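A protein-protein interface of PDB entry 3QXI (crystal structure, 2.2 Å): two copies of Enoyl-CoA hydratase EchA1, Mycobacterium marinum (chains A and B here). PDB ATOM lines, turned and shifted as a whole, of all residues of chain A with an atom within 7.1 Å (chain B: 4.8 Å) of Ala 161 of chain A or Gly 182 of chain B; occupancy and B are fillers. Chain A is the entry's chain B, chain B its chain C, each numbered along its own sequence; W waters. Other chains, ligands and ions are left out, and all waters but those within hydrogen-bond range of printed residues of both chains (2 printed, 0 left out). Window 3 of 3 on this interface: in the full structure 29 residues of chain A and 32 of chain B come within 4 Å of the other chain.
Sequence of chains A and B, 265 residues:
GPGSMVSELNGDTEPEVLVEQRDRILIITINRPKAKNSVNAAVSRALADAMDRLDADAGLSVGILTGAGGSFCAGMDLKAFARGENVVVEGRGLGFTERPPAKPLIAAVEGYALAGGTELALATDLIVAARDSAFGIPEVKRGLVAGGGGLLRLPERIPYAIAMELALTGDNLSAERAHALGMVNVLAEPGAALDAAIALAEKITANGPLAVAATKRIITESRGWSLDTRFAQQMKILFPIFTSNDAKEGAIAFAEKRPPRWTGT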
ATOM      1  N   PRO A 155      19.631 -28.211  -4.271  1.00  0.00           N
ATOM      2  CA  PRO A 155      18.195 -28.299  -4.580  1.00  0.00           C
ATOM      3  C   PRO A 155      17.332 -28.711  -3.383  1.00  0.00           C
ATOM      4  O   PRO A 155      16.089 -28.651  -3.449  1.00  0.00           O
ATOM      5  CB  PRO A 155      18.122 -29.385  -5.669  1.00  0.00           C
ATOM      6  CG  PRO A 155      19.469 -29.642  -6.105  1.00  0.00           C
ATOM      7  CD  PRO A 155      20.378 -29.287  -4.948  1.00  0.00           C
ATOM      8  N   ILE A 158      17.202 -24.687  -1.266  1.00  0.00           N
ATOM      9  CA  ILE A 158      16.565 -23.510  -1.875  1.00  0.00           C
ATOM     10  C   ILE A 158      15.618 -24.051  -2.943  1.00  0.00           C
ATOM     11  O   ILE A 158      15.682 -25.247  -3.238  1.00  0.00           O
ATOM     12  CB  ILE A 158      17.626 -22.551  -2.524  1.00  0.00           C
ATOM     13  CG1 ILE A 158      18.344 -23.193  -3.726  1.00  0.00           C
ATOM     14  CG2 ILE A 158      18.671 -22.106  -1.525  1.00  0.00           C
ATOM     15  CD1 ILE A 158      19.226 -22.191  -4.481  1.00  0.00           C
ATOM     16  N   PRO A 159      14.756 -23.205  -3.540  1.00  0.00           N
ATOM     17  CA  PRO A 159      13.848 -23.736  -4.552  1.00  0.00           C
ATOM     18  C   PRO A 159      14.579 -24.468  -5.699  1.00  0.00           C
ATOM     19  O   PRO A 159      15.599 -23.965  -6.214  1.00  0.00           O
ATOM     20  CB  PRO A 159      13.146 -22.479  -5.054  1.00  0.00           C
ATOM     21  CG  PRO A 159      13.042 -21.661  -3.805  1.00  0.00           C
ATOM     22  CD  PRO A 159      14.428 -21.791  -3.247  1.00  0.00           C
ATOM     23  N   TYR A 160      14.051 -25.644  -6.056  1.00  0.00           N
ATOM     24  CA  TYR A 160      14.625 -26.494  -7.110  1.00  0.00           C
ATOM     25  C   TYR A 160      15.078 -25.737  -8.366  1.00  0.00           C
ATOM     26  O   TYR A 160      16.209 -25.922  -8.821  1.00  0.00           O
ATOM     27  CB  TYR A 160      13.648 -27.634  -7.476  1.00  0.00           C
ATOM     28  CG  TYR A 160      14.156 -28.591  -8.518  1.00  0.00           C
ATOM     29  CD1 TYR A 160      14.827 -29.747  -8.142  1.00  0.00           C
ATOM     30  CD2 TYR A 160      13.971 -28.351  -9.865  1.00  0.00           C
ATOM     31  CE1 TYR A 160      15.297 -30.640  -9.062  1.00  0.00           C
ATOM     32  CE2 TYR A 160      14.450 -29.256 -10.825  1.00  0.00           C
ATOM     33  CZ  TYR A 160      15.116 -30.405 -10.396  1.00  0.00           C
ATOM     34  OH  TYR A 160      15.599 -31.330 -11.284  1.00  0.00           O
ATOM     35  N   ALA A 161      14.219 -24.885  -8.919  1.00  0.00           N
ATOM     36  CA  ALA A 161      14.543 -24.172 -10.164  1.00  0.00           C
ATOM     37  C   ALA A 161      15.674 -23.146 -10.011  1.00  0.00           C
ATOM     38  O   ALA A 161      16.439 -22.909 -10.964  1.00  0.00           O
ATOM     39  CB  ALA A 161      13.317 -23.526 -10.739  1.00  0.00           C
ATOM     40  N   ILE A 162      15.788 -22.540  -8.831  1.00  0.00           N
ATOM     41  CA  ILE A 162      16.860 -21.572  -8.592  1.00  0.00           C
ATOM     42  C   ILE A 162      18.179 -22.301  -8.397  1.00  0.00           C
ATOM     43  O   ILE A 162      19.190 -21.868  -8.934  1.00  0.00           O
ATOM     44  CB  ILE A 162      16.583 -20.639  -7.376  1.00  0.00           C
ATOM     45  CG1 ILE A 162      15.287 -19.828  -7.581  1.00  0.00           C
ATOM     46  CG2 ILE A 162      17.760 -19.707  -7.152  1.00  0.00           C
ATOM     47  CD1 ILE A 162      14.930 -18.902  -6.362  1.00  0.00           C
ATOM     48  N   ALA A 163      18.158 -23.412  -7.639  1.00  0.00           N
ATOM     49  CA  ALA A 163      19.305 -24.322  -7.598  1.00  0.00           C
ATOM     50  C   ALA A 163      19.780 -24.775  -8.984  1.00  0.00           C
ATOM     51  O   ALA A 163      20.980 -24.747  -9.273  1.00  0.00           O
ATOM     52  CB  ALA A 163      19.004 -25.535  -6.735  1.00  0.00           C
ATOM     53  N   MET A 164      18.851 -25.219  -9.826  1.00  0.00           N
ATOM     54  CA  MET A 164      19.183 -25.619 -11.206  1.00  0.00           C
ATOM     55  C   MET A 164      19.878 -24.458 -11.948  1.00  0.00           C
ATOM     56  O   MET A 164      20.935 -24.630 -12.570  1.00  0.00           O
ATOM     57  CB  MET A 164      17.918 -26.075 -11.956  1.00  0.00           C
ATOM     58  CG  MET A 164      18.137 -26.589 -13.419  1.00  0.00           C
ATOM     59  SD  MET A 164      19.149 -28.101 -13.476  1.00  0.00           S
ATOM     60  CE  MET A 164      17.875 -29.359 -13.158  1.00  0.00           C
ATOM     61  N   GLU A 165      19.255 -23.288 -11.878  1.00  0.00           N
ATOM     62  CA  GLU A 165      19.733 -22.099 -12.530  1.00  0.00           C
ATOM     63  C   GLU A 165      21.174 -21.787 -12.147  1.00  0.00           C
ATOM     64  O   GLU A 165      22.008 -21.622 -13.022  1.00  0.00           O
ATOM     65  CB  GLU A 165      18.827 -20.908 -12.200  1.00  0.00           C
ATOM     66  CG  GLU A 165      19.236 -19.634 -12.956  1.00  0.00           C
ATOM     67  CD  GLU A 165      18.494 -18.385 -12.452  1.00  0.00           C
ATOM     68  OE1 GLU A 165      17.412 -18.546 -11.824  1.00  0.00           O
ATOM     69  OE2 GLU A 165      18.991 -17.258 -12.687  1.00  0.00           O
ATOM     70  N   LEU A 166      21.440 -21.696 -10.850  1.00  0.00           N
ATOM     71  CA  LEU A 166      22.793 -21.459 -10.313  1.00  0.00           C
ATOM     72  C   LEU A 166      23.795 -22.513 -10.771  1.00  0.00           C
ATOM     73  O   LEU A 166      24.964 -22.189 -11.112  1.00  0.00           O
ATOM     74  CB  LEU A 166      22.746 -21.412  -8.778  1.00  0.00           C
ATOM     75  CG  LEU A 166      21.878 -20.281  -8.194  1.00  0.00           C
ATOM     76  CD1 LEU A 166      21.674 -20.439  -6.665  1.00  0.00           C
ATOM     77  CD2 LEU A 166      22.437 -18.872  -8.501  1.00  0.00           C
ATOM     78  N   ALA A 167      23.354 -23.772 -10.787  1.00  0.00           N
ATOM     79  CA  ALA A 167      24.225 -24.883 -11.214  1.00  0.00           C
ATOM     80  C   ALA A 167      24.614 -24.815 -12.705  1.00  0.00           C
ATOM     81  O   ALA A 167      25.769 -25.051 -13.075  1.00  0.00           O
ATOM     82  CB  ALA A 167      23.584 -26.208 -10.903  1.00  0.00           C
ATOM     83  N   LEU A 181      16.127 -17.032   0.698  1.00  0.00           N
ATOM     84  CA  LEU A 181      15.689 -18.307   0.170  1.00  0.00           C
ATOM     85  C   LEU A 181      15.705 -19.395   1.253  1.00  0.00           C
ATOM     86  O   LEU A 181      15.251 -20.532   1.002  1.00  0.00           O
ATOM     87  CB  LEU A 181      16.540 -18.697  -1.037  1.00  0.00           C
ATOM     88  CG  LEU A 181      16.362 -17.812  -2.249  1.00  0.00           C
ATOM     89  CD1 LEU A 181      17.359 -18.213  -3.304  1.00  0.00           C
ATOM     90  CD2 LEU A 181      14.865 -17.868  -2.756  1.00  0.00           C
ATOM     91  N   ASP B 125      13.443 -27.120 -17.454  1.00  0.00           N
ATOM     92  CA  ASP B 125      14.330 -26.828 -16.329  1.00  0.00           C
ATOM     93  C   ASP B 125      14.182 -25.430 -15.694  1.00  0.00           C
ATOM     94  O   ASP B 125      14.377 -25.274 -14.478  1.00  0.00           O
ATOM     95  CB  ASP B 125      15.785 -27.071 -16.735  1.00  0.00           C
ATOM     96  CG  ASP B 125      15.969 -28.425 -17.396  1.00  0.00           C
ATOM     97  OD1 ASP B 125      15.638 -29.442 -16.755  1.00  0.00           O
ATOM     98  OD2 ASP B 125      16.405 -28.469 -18.571  1.00  0.00           O
ATOM     99  N   LEU B 126      13.868 -24.421 -16.506  1.00  0.00           N
ATOM    100  CA  LEU B 126      13.894 -23.039 -16.034  1.00  0.00           C
ATOM    101  C   LEU B 126      12.714 -22.311 -16.666  1.00  0.00           C
ATOM    102  O   LEU B 126      12.397 -22.561 -17.841  1.00  0.00           O
ATOM    103  CB  LEU B 126      15.225 -22.342 -16.439  1.00  0.00           C
ATOM    104  CG  LEU B 126      16.539 -23.022 -15.953  1.00  0.00           C
ATOM    105  CD1 LEU B 126      17.801 -22.640 -16.741  1.00  0.00           C
ATOM    106  CD2 LEU B 126      16.763 -22.832 -14.407  1.00  0.00           C
ATOM    107  N   ARG B 157       8.482 -27.678  -6.787  1.00  0.00           N
ATOM    108  CA  ARG B 157       8.947 -26.345  -7.200  1.00  0.00           C
ATOM    109  C   ARG B 157       8.649 -25.204  -6.254  1.00  0.00           C
ATOM    110  O   ARG B 157       9.331 -24.179  -6.316  1.00  0.00           O
ATOM    111  CB  ARG B 157       8.396 -25.996  -8.583  1.00  0.00           C
ATOM    112  CG  ARG B 157       8.682 -27.060  -9.608  1.00  0.00           C
ATOM    113  CD  ARG B 157      10.161 -27.077 -10.005  1.00  0.00           C
ATOM    114  NE  ARG B 157      10.344 -27.990 -11.139  1.00  0.00           N
ATOM    115  CZ  ARG B 157      10.571 -29.292 -11.010  1.00  0.00           C
ATOM    116  NH1 ARG B 157      10.676 -29.825  -9.807  1.00  0.00           N
ATOM    117  NH2 ARG B 157      10.727 -30.055 -12.086  1.00  0.00           N
ATOM    118  N   ALA B 178       4.507 -16.858  -8.503  1.00  0.00           N
ATOM    119  CA  ALA B 178       5.380 -18.019  -8.830  1.00  0.00           C
ATOM    120  C   ALA B 178       6.851 -17.626  -8.774  1.00  0.00           C
ATOM    121  O   ALA B 178       7.689 -18.465  -8.478  1.00  0.00           O
ATOM    122  CB  ALA B 178       5.045 -18.643 -10.230  1.00  0.00           C
ATOM    123  N   HIS B 179       7.165 -16.362  -9.057  1.00  0.00           N
ATOM    124  CA  HIS B 179       8.559 -15.911  -8.982  1.00  0.00           C
ATOM    125  C   HIS B 179       8.987 -15.770  -7.516  1.00  0.00           C
ATOM    126  O   HIS B 179      10.089 -16.192  -7.128  1.00  0.00           O
ATOM    127  CB  HIS B 179       8.783 -14.621  -9.806  1.00  0.00           C
ATOM    128  CG  HIS B 179      10.118 -13.982  -9.585  1.00  0.00           C
ATOM    129  ND1 HIS B 179      10.312 -12.971  -8.671  1.00  0.00           N
ATOM    130  CD2 HIS B 179      11.334 -14.249 -10.120  1.00  0.00           C
ATOM    131  CE1 HIS B 179      11.589 -12.634  -8.664  1.00  0.00           C
ATOM    132  NE2 HIS B 179      12.226 -13.394  -9.537  1.00  0.00           N
ATOM    133  N   ALA B 180       8.097 -15.219  -6.689  1.00  0.00           N
ATOM    134  CA  ALA B 180       8.378 -15.034  -5.247  1.00  0.00           C
ATOM    135  C   ALA B 180       8.512 -16.405  -4.587  1.00  0.00           C
ATOM    136  O   ALA B 180       9.286 -16.591  -3.665  1.00  0.00           O
ATOM    137  CB  ALA B 180       7.266 -14.211  -4.577  1.00  0.00           C
ATOM    138  N   LEU B 181       7.731 -17.368  -5.071  1.00  0.00           N
ATOM    139  CA  LEU B 181       7.818 -18.722  -4.567  1.00  0.00           C
ATOM    140  C   LEU B 181       9.020 -19.516  -5.106  1.00  0.00           C
ATOM    141  O   LEU B 181       9.320 -20.606  -4.621  1.00  0.00           O
ATOM    142  CB  LEU B 181       6.500 -19.441  -4.855  1.00  0.00           C
ATOM    143  CG  LEU B 181       5.328 -18.855  -4.085  1.00  0.00           C
ATOM    144  CD1 LEU B 181       4.040 -19.487  -4.541  1.00  0.00           C
ATOM    145  CD2 LEU B 181       5.500 -19.038  -2.569  1.00  0.00           C
ATOM    146  N   GLY B 182       9.713 -18.978  -6.098  1.00  0.00           N
ATOM    147  CA  GLY B 182      10.872 -19.660  -6.632  1.00  0.00           C
ATOM    148  C   GLY B 182      10.618 -20.608  -7.774  1.00  0.00           C
ATOM    149  O   GLY B 182      11.524 -21.295  -8.195  1.00  0.00           O
ATOM    150  N   MET B 183       9.395 -20.637  -8.292  1.00  0.00           N
ATOM    151  CA  MET B 183       9.090 -21.427  -9.489  1.00  0.00           C
ATOM    152  C   MET B 183       9.537 -20.741 -10.782  1.00  0.00           C
ATOM    153  O   MET B 183      10.016 -21.399 -11.682  1.00  0.00           O
ATOM    154  CB  MET B 183       7.604 -21.699  -9.583  1.00  0.00           C
ATOM    155  CG  MET B 183       7.178 -22.495 -10.819  1.00  0.00           C
ATOM    156  SD  MET B 183       5.410 -22.828 -10.716  1.00  0.00           S
ATOM    157  CE  MET B 183       4.894 -22.924 -12.428  1.00  0.00           C
ATOM    158  N   VAL B 184       9.286 -19.447 -10.902  1.00  0.00           N
ATOM    159  CA  VAL B 184       9.701 -18.690 -12.068  1.00  0.00           C
ATOM    160  C   VAL B 184      11.103 -18.088 -11.777  1.00  0.00           C
ATOM    161  O   VAL B 184      11.301 -17.377 -10.779  1.00  0.00           O
ATOM    162  CB  VAL B 184       8.652 -17.601 -12.415  1.00  0.00           C
ATOM    163  CG1 VAL B 184       9.247 -16.508 -13.353  1.00  0.00           C
ATOM    164  CG2 VAL B 184       7.358 -18.253 -13.030  1.00  0.00           C
ATOM    165  N   ASN B 185      12.072 -18.373 -12.637  1.00  0.00           N
ATOM    166  CA  ASN B 185      13.440 -17.866 -12.437  1.00  0.00           C
ATOM    167  C   ASN B 185      13.616 -16.407 -12.803  1.00  0.00           C
ATOM    168  O   ASN B 185      14.396 -15.691 -12.151  1.00  0.00           O
ATOM    169  CB  ASN B 185      14.441 -18.677 -13.237  1.00  0.00           C
ATOM    170  CG  ASN B 185      14.409 -20.152 -12.891  1.00  0.00           C
ATOM    171  OD1 ASN B 185      13.570 -20.885 -13.383  1.00  0.00           O
ATOM    172  ND2 ASN B 185      15.336 -20.591 -12.050  1.00  0.00           N
HETATM  173  O   HOH W   1      11.554 -24.101  -7.945  1.00  0.00           O
HETATM  174  O   HOH W   2      16.157 -16.625 -10.258  1.00  0.00           O
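Position printed for both chains: 181. Of the 9 pairs that touch across the chains among the printed residues, none has its exchanged pair printed and touching as well.
Ala 161 of chain A touches just these residues of chain B: Leu 126, Gly 182 and Asn 185. Of chain A, only Pro 159 and Ala 161 come within 4 Å of Gly 182 of chain B. Of the printed residues of chain B, Glu 165 of chain A touches Leu 126 (3.6 Å) and Asn 185 (2.9 Å). Of the printed residues of chain B, Tyr 160 of chain A touches Arg 157 (3.6 Å). The nearest residue of chain B that does not touch Ala 161 of chain A is Met 183 of chain B (4.04 Å).
Printed residues of chain A that touch a printed residue of chain B: Pro 159, Tyr 160, Ala 161, Ile 162 and Glu 165. Of the 11 printed residues of chain B, 5 touch a printed residue of chain A. Hydrophobic or aromatic side chains of chain B that line the printed part of chain A: Leu 126. Among the printed residues, 9 pairs touch across the chains.
Pro 159 of chain A touches Leu 181 of chain B. CB of Pro 159 of chain A touches O of Gly 182 of chain B, 3.7 Å away. NH1 of Arg 157 of chain B touches CD2 of Tyr 160 of chain A, at 3.6 Å. Leu 126 of chain B touches Ala 161 of chain A. Gly 182 of chain B touches Ala 161 of chain A. N of Ile 162 of chain A touches ND2 of Asn 185 of chain B, 3.8 Å away. Glu 165 of chain A touches Leu 126 of chain B (N to CD2, 3.6 Å).
Water W2 lies within hydrogen-bond range of O of Asn 185 of chain B (2.7 Å) and OE1 of Glu 165 of chain A (2.8 Å). Water W1 lies within hydrogen-bond range of O of Arg 157 of chain B (2.8 Å), O of Gly 182 of chain B (2.8 Å), N of Ala 161 of chain A (2.9 Å) and N of Tyr 160 of chain A (3.5 Å).
The backbone carbonyl oxygen (O) of Ala 161 of chain A lies within hydrogen-bond range of the side-chain amide nitrogen (ND2) of Asn 185 of chain B (2.8 Å). The side-chain amide nitrogen of Asn 185 of chain B is in hydrogen-bond range of the side-chain carboxylate of Glu 165 of chain A, 2.9 Å away.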
